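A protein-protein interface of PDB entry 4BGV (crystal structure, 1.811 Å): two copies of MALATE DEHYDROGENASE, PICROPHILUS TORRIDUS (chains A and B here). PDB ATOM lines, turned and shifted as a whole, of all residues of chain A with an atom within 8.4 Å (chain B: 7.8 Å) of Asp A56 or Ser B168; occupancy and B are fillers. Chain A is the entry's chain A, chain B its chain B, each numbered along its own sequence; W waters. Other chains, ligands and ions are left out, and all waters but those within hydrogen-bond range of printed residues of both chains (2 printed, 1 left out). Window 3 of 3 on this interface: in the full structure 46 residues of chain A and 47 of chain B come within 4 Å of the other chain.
The side-chain carboxylate (OD1) of Asp A56 lies within hydrogen-bond range of the backbone NH (N) of Phe B169, at 2.9 Å.
NH2 of Arg B158 is in hydrogen-bond range of O of Pro A51 (3.5 Å).
OG of Ser B168 is in hydrogen-bond range of OD2 of Asp A56.
Arg A2 touches none of the printed residues of chain B.
Of the printed residues of chain B, Leu A47 touches Gln B163 and Phe B169.
Of the printed residues of chain B, Ala A50 touches Phe B169 (3.4 Å).
Of the printed residues of chain B, Pro A51 touches Arg B158 (3.4 Å) and Phe B169 (3.8 Å).
Of chain B, only Ser B168 (2.7 Å) and Phe B169 (2.9 Å) come within 4 Å of Asp A56.
Of the printed residues of chain A, Gln B163 touches Leu A47.
Ser B168 touches just one residue of chain A: Asp A56 (2.7 Å).
The nearest residue of chain B that does not touch Asp A56 is Glu B170 (4.3 Å).
The nearest residue of chain A that does not touch Ser B168 is Gly A54 (6.0 Å).
The guanidinium group (NE) of Arg A2 sits close to the backbone carbonyl oxygen (O) of Asp A56, at 3.5 Å.
The backbone carbonyl oxygen (O) of Val B172 lies within hydrogen-bond range of the guanidinium group (NE) of Arg B158, at 2.8 Å.
N of Glu B170 lies within hydrogen-bond range of OG of Ser B168, at 3.0 Å.
The backbone carbonyl oxygen of Phe B169 sits at hydrogen-bond distance from the guanidinium group of Arg B158 (2.9 Å).
CD2 of Leu A47 touches OE1 of Gln B163, 3.2 Å away.
CZ of Phe B169 touches CD1 of Leu A47, at 3.8 Å.
CD2 of Phe B169 touches CB of Ala A50, 3.4 Å away.
CA of Pro A51 touches CB of Phe B169, 3.8 Å away.
Tyr A55 touches Phe B169.
No position is printed for both chains.
Of the 8 pairs that touch across the chains among the printed residues, none has its exchanged pair printed and touching as well.
Of the 15 printed residues of chain A, 5 touch a printed residue of chain B.
Along chain B the printed residues that touch a printed residue of chain A span positions 158 to 169.
Among the printed residues, no Asp or Glu carboxylate lies within 4 Å of a Lys or Arg side-chain nitrogen of the other chain.
Water W2 lies within hydrogen-bond range of the backbone carbonyl oxygen of Pro A51 (2.8 Å), the backbone carbonyl oxygen of Ala A50 (3.3 Å) and the backbone NH of Glu B170 (3.4 Å).
Water W1 lies within hydrogen-bond range of the side-chain carboxylate of Asp A56 (2.9 Å), the backbone carbonyl oxygen of Gly A54 (2.9 Å) and the backbone NH of Glu B170 (3.2 Å).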
ATOM      1  N   ARG A   2      -3.909   3.605 -21.967  1.00  0.00           N
ATOM      2  CA  ARG A   2      -4.953   2.714 -22.468  1.00  0.00           C
ATOM      3  C   ARG A   2      -4.653   2.351 -23.920  1.00  0.00           C
ATOM      4  O   ARG A   2      -4.006   3.108 -24.640  1.00  0.00           O
ATOM      5  CB  ARG A   2      -6.330   3.390 -22.419  1.00  0.00           C
ATOM      6  CG  ARG A   2      -6.915   3.681 -21.023  1.00  0.00           C
ATOM      7  CD  ARG A   2      -8.092   4.661 -21.147  1.00  0.00           C
ATOM      8  NE  ARG A   2      -8.064   5.665 -20.084  1.00  0.00           N
ATOM      9  CZ  ARG A   2      -8.516   6.899 -20.219  1.00  0.00           C
ATOM     10  NH1 ARG A   2      -9.032   7.300 -21.380  1.00  0.00           N
ATOM     11  NH2 ARG A   2      -8.451   7.734 -19.195  1.00  0.00           N
ATOM     12  N   ALA A  22     -16.787  -0.149 -25.197  1.00  0.00           N
ATOM     13  CA  ALA A  22     -16.839   0.794 -24.065  1.00  0.00           C
ATOM     14  C   ALA A  22     -17.346   0.103 -22.808  1.00  0.00           C
ATOM     15  O   ALA A  22     -16.737   0.216 -21.739  1.00  0.00           O
ATOM     16  CB  ALA A  22     -17.708   2.008 -24.400  1.00  0.00           C
ATOM     17  N   GLN A  25     -14.892  -2.018 -21.437  1.00  0.00           N
ATOM     18  CA  GLN A  25     -13.729  -1.200 -21.061  1.00  0.00           C
ATOM     19  C   GLN A  25     -12.440  -1.607 -21.773  1.00  0.00           C
ATOM     20  O   GLN A  25     -11.342  -1.615 -21.187  1.00  0.00           O
ATOM     21  CB  GLN A  25     -13.580  -1.177 -19.531  1.00  0.00           C
ATOM     22  CG  GLN A  25     -14.839  -0.627 -18.872  1.00  0.00           C
ATOM     23  CD  GLN A  25     -14.757  -0.451 -17.358  1.00  0.00           C
ATOM     24  OE1 GLN A  25     -13.708  -0.624 -16.746  1.00  0.00           O
ATOM     25  NE2 GLN A  25     -15.886  -0.093 -16.754  1.00  0.00           N
ATOM     26  N   GLY A  27     -10.707  -0.201 -24.300  1.00  0.00           N
ATOM     27  CA  GLY A  27      -9.719   0.842 -24.520  1.00  0.00           C
ATOM     28  C   GLY A  27     -10.409   2.076 -25.063  1.00  0.00           C
ATOM     29  O   GLY A  27     -11.624   2.093 -25.166  1.00  0.00           O
ATOM     30  N   ASP A  28      -9.637   3.103 -25.396  1.00  0.00           N
ATOM     31  CA  ASP A  28     -10.210   4.281 -26.050  1.00  0.00           C
ATOM     32  C   ASP A  28     -10.710   3.893 -27.432  1.00  0.00           C
ATOM     33  O   ASP A  28     -10.147   3.012 -28.083  1.00  0.00           O
ATOM     34  CB  ASP A  28      -9.163   5.389 -26.156  1.00  0.00           C
ATOM     35  CG  ASP A  28      -8.712   5.893 -24.790  1.00  0.00           C
ATOM     36  OD1 ASP A  28      -9.552   5.967 -23.862  1.00  0.00           O
ATOM     37  OD2 ASP A  28      -7.517   6.214 -24.643  1.00  0.00           O
ATOM     38  N   LEU A  47     -20.503   8.098 -25.481  1.00  0.00           N
ATOM     39  CA  LEU A  47     -19.757   8.732 -24.390  1.00  0.00           C
ATOM     40  C   LEU A  47     -20.680   9.272 -23.295  1.00  0.00           C
ATOM     41  O   LEU A  47     -20.365   9.194 -22.106  1.00  0.00           O
ATOM     42  CB  LEU A  47     -18.886   9.881 -24.908  1.00  0.00           C
ATOM     43  CG  LEU A  47     -17.972  10.512 -23.860  1.00  0.00           C
ATOM     44  CD1 LEU A  47     -16.930   9.493 -23.398  1.00  0.00           C
ATOM     45  CD2 LEU A  47     -17.309  11.770 -24.429  1.00  0.00           C
ATOM     46  N   ALA A  50     -21.387   7.131 -20.312  1.00  0.00           N
ATOM     47  CA  ALA A  50     -20.272   6.802 -19.405  1.00  0.00           C
ATOM     48  C   ALA A  50     -20.537   7.009 -17.896  1.00  0.00           C
ATOM     49  O   ALA A  50     -20.158   6.155 -17.079  1.00  0.00           O
ATOM     50  CB  ALA A  50     -18.994   7.546 -19.833  1.00  0.00           C
ATOM     51  N   PRO A  51     -21.161   8.140 -17.507  1.00  0.00           N
ATOM     52  CA  PRO A  51     -21.403   8.286 -16.067  1.00  0.00           C
ATOM     53  C   PRO A  51     -22.275   7.173 -15.458  1.00  0.00           C
ATOM     54  O   PRO A  51     -22.065   6.818 -14.294  1.00  0.00           O
ATOM     55  CB  PRO A  51     -22.092   9.655 -15.960  1.00  0.00           C
ATOM     56  CG  PRO A  51     -21.550  10.423 -17.151  1.00  0.00           C
ATOM     57  CD  PRO A  51     -21.465   9.388 -18.242  1.00  0.00           C
ATOM     58  N   TRP A  53     -22.692   3.944 -16.942  1.00  0.00           N
ATOM     59  CA  TRP A  53     -22.047   2.648 -17.174  1.00  0.00           C
ATOM     60  C   TRP A  53     -20.765   2.508 -16.343  1.00  0.00           C
ATOM     61  O   TRP A  53     -20.425   1.417 -15.872  1.00  0.00           O
ATOM     62  CB  TRP A  53     -21.671   2.479 -18.646  1.00  0.00           C
ATOM     63  CG  TRP A  53     -22.730   1.949 -19.592  1.00  0.00           C
ATOM     64  CD1 TRP A  53     -23.321   2.625 -20.625  1.00  0.00           C
ATOM     65  CD2 TRP A  53     -23.270   0.621 -19.623  1.00  0.00           C
ATOM     66  NE1 TRP A  53     -24.211   1.807 -21.284  1.00  0.00           N
ATOM     67  CE2 TRP A  53     -24.200   0.572 -20.690  1.00  0.00           C
ATOM     68  CE3 TRP A  53     -23.065  -0.528 -18.848  1.00  0.00           C
ATOM     69  CZ2 TRP A  53     -24.910  -0.584 -21.010  1.00  0.00           C
ATOM     70  CZ3 TRP A  53     -23.782  -1.676 -19.157  1.00  0.00           C
ATOM     71  CH2 TRP A  53     -24.690  -1.696 -20.234  1.00  0.00           C
ATOM     72  N   GLY A  54     -20.024   3.601 -16.206  1.00  0.00           N
ATOM     73  CA  GLY A  54     -18.777   3.567 -15.471  1.00  0.00           C
ATOM     74  C   GLY A  54     -17.488   3.520 -16.276  1.00  0.00           C
ATOM     75  O   GLY A  54     -16.422   3.460 -15.678  1.00  0.00           O
ATOM     76  N   TYR A  55     -17.551   3.572 -17.605  1.00  0.00           N
ATOM     77  CA  TYR A  55     -16.309   3.535 -18.393  1.00  0.00           C
ATOM     78  C   TYR A  55     -15.597   4.876 -18.503  1.00  0.00           C
ATOM     79  O   TYR A  55     -16.179   5.868 -18.938  1.00  0.00           O
ATOM     80  CB  TYR A  55     -16.505   2.902 -19.785  1.00  0.00           C
ATOM     81  CG  TYR A  55     -17.743   3.299 -20.581  1.00  0.00           C
ATOM     82  CD1 TYR A  55     -17.792   4.494 -21.305  1.00  0.00           C
ATOM     83  CD2 TYR A  55     -18.831   2.435 -20.668  1.00  0.00           C
ATOM     84  CE1 TYR A  55     -18.912   4.833 -22.064  1.00  0.00           C
ATOM     85  CE2 TYR A  55     -19.944   2.765 -21.414  1.00  0.00           C
ATOM     86  CZ  TYR A  55     -19.988   3.945 -22.108  1.00  0.00           C
ATOM     87  OH  TYR A  55     -21.119   4.222 -22.837  1.00  0.00           O
ATOM     88  N   ASP A  56     -14.333   4.909 -18.076  1.00  0.00           N
ATOM     89  CA  ASP A  56     -13.530   6.126 -18.161  1.00  0.00           C
ATOM     90  C   ASP A  56     -12.631   6.025 -19.386  1.00  0.00           C
ATOM     91  O   ASP A  56     -11.458   5.644 -19.295  1.00  0.00           O
ATOM     92  CB  ASP A  56     -12.710   6.328 -16.888  1.00  0.00           C
ATOM     93  CG  ASP A  56     -13.547   6.891 -15.745  1.00  0.00           C
ATOM     94  OD1 ASP A  56     -14.429   7.722 -16.031  1.00  0.00           O
ATOM     95  OD2 ASP A  56     -13.322   6.506 -14.581  1.00  0.00           O
ATOM     96  N   LEU A  57     -13.213   6.347 -20.537  1.00  0.00           N
ATOM     97  CA  LEU A  57     -12.558   6.200 -21.831  1.00  0.00           C
ATOM     98  C   LEU A  57     -12.743   7.452 -22.677  1.00  0.00           C
ATOM     99  O   LEU A  57     -13.651   8.249 -22.452  1.00  0.00           O
ATOM    100  CB  LEU A  57     -13.171   5.025 -22.610  1.00  0.00           C
ATOM    101  CG  LEU A  57     -13.114   3.664 -21.920  1.00  0.00           C
ATOM    102  CD1 LEU A  57     -14.022   2.687 -22.634  1.00  0.00           C
ATOM    103  CD2 LEU A  57     -11.667   3.142 -21.862  1.00  0.00           C
ATOM    104  N   ASP A  58     -11.851   7.613 -23.642  1.00  0.00           N
ATOM    105  CA  ASP A  58     -11.954   8.673 -24.619  1.00  0.00           C
ATOM    106  C   ASP A  58     -12.671   8.029 -25.789  1.00  0.00           C
ATOM    107  O   ASP A  58     -12.237   6.994 -26.305  1.00  0.00           O
ATOM    108  CB  ASP A  58     -10.540   9.116 -24.993  1.00  0.00           C
ATOM    109  CG  ASP A  58     -10.517  10.295 -25.930  1.00  0.00           C
ATOM    110  OD1 ASP A  58     -11.557  10.978 -26.066  1.00  0.00           O
ATOM    111  OD2 ASP A  58      -9.443  10.537 -26.528  1.00  0.00           O
ATOM    112  N   ILE A  59     -13.804   8.599 -26.177  1.00  0.00           N
ATOM    113  CA  ILE A  59     -14.572   8.050 -27.283  1.00  0.00           C
ATOM    114  C   ILE A  59     -14.859   9.199 -28.242  1.00  0.00           C
ATOM    115  O   ILE A  59     -15.514  10.177 -27.865  1.00  0.00           O
ATOM    116  CB  ILE A  59     -15.880   7.408 -26.773  1.00  0.00           C
ATOM    117  CG1 ILE A  59     -15.550   6.349 -25.698  1.00  0.00           C
ATOM    118  CG2 ILE A  59     -16.669   6.816 -27.931  1.00  0.00           C
ATOM    119  CD1 ILE A  59     -16.754   5.639 -25.142  1.00  0.00           C
ATOM    120  N   ARG B 158     -23.051  15.502 -16.413  1.00  0.00           N
ATOM    121  CA  ARG B 158     -21.854  14.891 -15.834  1.00  0.00           C
ATOM    122  C   ARG B 158     -20.756  14.658 -16.864  1.00  0.00           C
ATOM    123  O   ARG B 158     -19.585  14.876 -16.579  1.00  0.00           O
ATOM    124  CB  ARG B 158     -22.197  13.564 -15.153  1.00  0.00           C
ATOM    125  CG  ARG B 158     -23.014  13.715 -13.893  1.00  0.00           C
ATOM    126  CD  ARG B 158     -23.534  12.357 -13.438  1.00  0.00           C
ATOM    127  NE  ARG B 158     -22.456  11.501 -12.945  1.00  0.00           N
ATOM    128  CZ  ARG B 158     -22.624  10.223 -12.613  1.00  0.00           C
ATOM    129  NH1 ARG B 158     -23.834   9.662 -12.744  1.00  0.00           N
ATOM    130  NH2 ARG B 158     -21.587   9.507 -12.161  1.00  0.00           N
ATOM    131  N   LEU B 161     -19.087  18.011 -17.651  1.00  0.00           N
ATOM    132  CA  LEU B 161     -18.323  18.457 -16.491  1.00  0.00           C
ATOM    133  C   LEU B 161     -17.040  17.643 -16.372  1.00  0.00           C
ATOM    134  O   LEU B 161     -15.977  18.191 -16.095  1.00  0.00           O
ATOM    135  CB  LEU B 161     -19.143  18.315 -15.196  1.00  0.00           C
ATOM    136  CG  LEU B 161     -20.197  19.402 -14.928  1.00  0.00           C
ATOM    137  CD1 LEU B 161     -21.039  19.040 -13.691  1.00  0.00           C
ATOM    138  CD2 LEU B 161     -19.566  20.792 -14.749  1.00  0.00           C
ATOM    139  N   ALA B 162     -17.156  16.330 -16.561  1.00  0.00           N
ATOM    140  CA  ALA B 162     -15.998  15.451 -16.427  1.00  0.00           C
ATOM    141  C   ALA B 162     -14.939  15.740 -17.483  1.00  0.00           C
ATOM    142  O   ALA B 162     -13.746  15.719 -17.192  1.00  0.00           O
ATOM    143  CB  ALA B 162     -16.427  13.991 -16.491  1.00  0.00           C
ATOM    144  N   GLN B 163     -15.368  15.997 -18.714  1.00  0.00           N
ATOM    145  CA  GLN B 163     -14.418  16.330 -19.773  1.00  0.00           C
ATOM    146  C   GLN B 163     -13.753  17.687 -19.545  1.00  0.00           C
ATOM    147  O   GLN B 163     -12.574  17.886 -19.849  1.00  0.00           O
ATOM    148  CB  GLN B 163     -15.122  16.368 -21.121  1.00  0.00           C
ATOM    149  CG  GLN B 163     -15.562  15.025 -21.633  1.00  0.00           C
ATOM    150  CD  GLN B 163     -16.113  15.148 -23.036  1.00  0.00           C
ATOM    151  OE1 GLN B 163     -15.653  14.468 -23.944  1.00  0.00           O
ATOM    152  NE2 GLN B 163     -17.081  16.059 -23.226  1.00  0.00           N
ATOM    153  N   LEU B 165     -13.212  19.157 -16.657  1.00  0.00           N
ATOM    154  CA  LEU B 165     -12.351  19.130 -15.475  1.00  0.00           C
ATOM    155  C   LEU B 165     -11.333  17.995 -15.518  1.00  0.00           C
ATOM    156  O   LEU B 165     -10.471  17.883 -14.630  1.00  0.00           O
ATOM    157  CB  LEU B 165     -13.197  19.039 -14.208  1.00  0.00           C
ATOM    158  CG  LEU B 165     -13.858  20.370 -13.818  1.00  0.00           C
ATOM    159  CD1 LEU B 165     -14.905  20.139 -12.740  1.00  0.00           C
ATOM    160  CD2 LEU B 165     -12.802  21.371 -13.341  1.00  0.00           C
ATOM    161  N   ASN B 166     -11.433  17.177 -16.565  1.00  0.00           N
ATOM    162  CA  ASN B 166     -10.550  16.029 -16.761  1.00  0.00           C
ATOM    163  C   ASN B 166     -10.527  15.122 -15.529  1.00  0.00           C
ATOM    164  O   ASN B 166      -9.463  14.872 -14.952  1.00  0.00           O
ATOM    165  CB  ASN B 166      -9.133  16.490 -17.138  1.00  0.00           C
ATOM    166  CG  ASN B 166      -8.255  15.350 -17.655  1.00  0.00           C
ATOM    167  OD1 ASN B 166      -8.747  14.352 -18.179  1.00  0.00           O
ATOM    168  ND2 ASN B 166      -6.944  15.502 -17.500  1.00  0.00           N
ATOM    169  N   VAL B 167     -11.710  14.653 -15.131  1.00  0.00           N
ATOM    170  CA  VAL B 167     -11.858  13.743 -13.992  1.00  0.00           C
ATOM    171  C   VAL B 167     -12.739  12.567 -14.396  1.00  0.00           C
ATOM    172  O   VAL B 167     -13.449  12.642 -15.394  1.00  0.00           O
ATOM    173  CB  VAL B 167     -12.489  14.442 -12.769  1.00  0.00           C
ATOM    174  CG1 VAL B 167     -11.560  15.531 -12.229  1.00  0.00           C
ATOM    175  CG2 VAL B 167     -13.862  15.017 -13.143  1.00  0.00           C
ATOM    176  N   SER B 168     -12.675  11.475 -13.633  1.00  0.00           N
ATOM    177  CA  SER B 168     -13.520  10.297 -13.867  1.00  0.00           C
ATOM    178  C   SER B 168     -15.008  10.644 -13.922  1.00  0.00           C
ATOM    179  O   SER B 168     -15.496  11.440 -13.106  1.00  0.00           O
ATOM    180  CB  SER B 168     -13.342   9.284 -12.724  1.00  0.00           C
ATOM    181  OG  SER B 168     -14.304   8.237 -12.828  1.00  0.00           O
ATOM    182  N   PHE B 169     -15.735  10.007 -14.841  1.00  0.00           N
ATOM    183  CA  PHE B 169     -17.186  10.199 -14.911  1.00  0.00           C
ATOM    184  C   PHE B 169     -17.871   9.748 -13.630  1.00  0.00           C
ATOM    185  O   PHE B 169     -18.958  10.222 -13.291  1.00  0.00           O
ATOM    186  CB  PHE B 169     -17.783   9.435 -16.100  1.00  0.00           C
ATOM    187  CG  PHE B 169     -17.277   9.896 -17.425  1.00  0.00           C
ATOM    188  CD1 PHE B 169     -17.599  11.153 -17.895  1.00  0.00           C
ATOM    189  CD2 PHE B 169     -16.485   9.079 -18.202  1.00  0.00           C
ATOM    190  CE1 PHE B 169     -17.132  11.597 -19.108  1.00  0.00           C
ATOM    191  CE2 PHE B 169     -16.022   9.508 -19.435  1.00  0.00           C
ATOM    192  CZ  PHE B 169     -16.351  10.770 -19.891  1.00  0.00           C
ATOM    193  N   GLU B 170     -17.234   8.831 -12.910  1.00  0.00           N
ATOM    194  CA  GLU B 170     -17.852   8.292 -11.706  1.00  0.00           C
ATOM    195  C   GLU B 170     -17.911   9.312 -10.566  1.00  0.00           C
ATOM    196  O   GLU B 170     -18.766   9.211  -9.682  1.00  0.00           O
ATOM    197  CB  GLU B 170     -17.126   7.022 -11.244  1.00  0.00           C
ATOM    198  CG  GLU B 170     -17.765   6.365 -10.038  1.00  0.00           C
ATOM    199  CD  GLU B 170     -17.201   4.998  -9.753  1.00  0.00           C
ATOM    200  OE1 GLU B 170     -16.215   4.609 -10.422  1.00  0.00           O
ATOM    201  OE2 GLU B 170     -17.758   4.308  -8.867  1.00  0.00           O
ATOM    202  N   ASP B 171     -17.012  10.293 -10.574  1.00  0.00           N
ATOM    203  CA  ASP B 171     -16.892  11.192  -9.423  1.00  0.00           C
ATOM    204  C   ASP B 171     -17.594  12.540  -9.596  1.00  0.00           C
ATOM    205  O   ASP B 171     -17.660  13.341  -8.656  1.00  0.00           O
ATOM    206  CB  ASP B 171     -15.408  11.354  -9.065  1.00  0.00           C
ATOM    207  CG  ASP B 171     -14.789  10.038  -8.638  1.00  0.00           C
ATOM    208  OD1 ASP B 171     -15.490   9.267  -7.937  1.00  0.00           O
ATOM    209  OD2 ASP B 171     -13.645   9.738  -9.031  1.00  0.00           O
ATOM    210  N   VAL B 172     -18.116  12.782 -10.798  1.00  0.00           N
ATOM    211  CA  VAL B 172     -18.878  14.002 -11.067  1.00  0.00           C
ATOM    212  C   VAL B 172     -20.337  13.779 -10.700  1.00  0.00           C
ATOM    213  O   VAL B 172     -20.916  12.747 -11.016  1.00  0.00           O
ATOM    214  CB  VAL B 172     -18.817  14.401 -12.558  1.00  0.00           C
ATOM    215  CG1 VAL B 172     -19.718  15.604 -12.820  1.00  0.00           C
ATOM    216  CG2 VAL B 172     -17.404  14.735 -12.969  1.00  0.00           C
ATOM    217  N   ASN B 173     -20.933  14.760 -10.037  1.00  0.00           N
ATOM    218  CA  ASN B 173     -22.334  14.699  -9.680  1.00  0.00           C
ATOM    219  C   ASN B 173     -23.002  15.974 -10.147  1.00  0.00           C
ATOM    220  O   ASN B 173     -22.548  17.075  -9.831  1.00  0.00           O
ATOM    221  CB  ASN B 173     -22.467  14.533  -8.175  1.00  0.00           C
ATOM    222  CG  ASN B 173     -21.823  13.262  -7.683  1.00  0.00           C
ATOM    223  OD1 ASN B 173     -22.374  12.168  -7.865  1.00  0.00           O
ATOM    224  ND2 ASN B 173     -20.640  13.386  -7.069  1.00  0.00           N
ATOM    225  N   VAL B 193     -17.548  17.570  -7.635  1.00  0.00           N
ATOM    226  CA  VAL B 193     -16.654  16.476  -8.003  1.00  0.00           C
ATOM    227  C   VAL B 193     -16.195  15.869  -6.691  1.00  0.00           C
ATOM    228  O   VAL B 193     -15.470  16.519  -5.933  1.00  0.00           O
ATOM    229  CB  VAL B 193     -15.410  16.976  -8.775  1.00  0.00           C
ATOM    230  CG1 VAL B 193     -14.483  15.792  -9.095  1.00  0.00           C
ATOM    231  CG2 VAL B 193     -15.818  17.642 -10.071  1.00  0.00           C
ATOM    232  N   SER B 194     -16.640  14.642  -6.412  1.00  0.00           N
ATOM    233  CA  SER B 194     -16.356  13.965  -5.145  1.00  0.00           C
ATOM    234  C   SER B 194     -16.637  14.867  -3.936  1.00  0.00           C
ATOM    235  O   SER B 194     -15.893  14.852  -2.950  1.00  0.00           O
ATOM    236  CB  SER B 194     -14.910  13.470  -5.105  1.00  0.00           C
ATOM    237  OG  SER B 194     -14.673  12.510  -6.132  1.00  0.00           O
HETATM  238  O   HOH W   1     -16.522   6.229 -14.692  1.00  0.00           O
HETATM  239  O   HOH W   2     -19.297   6.349 -13.891  1.00  0.00           O
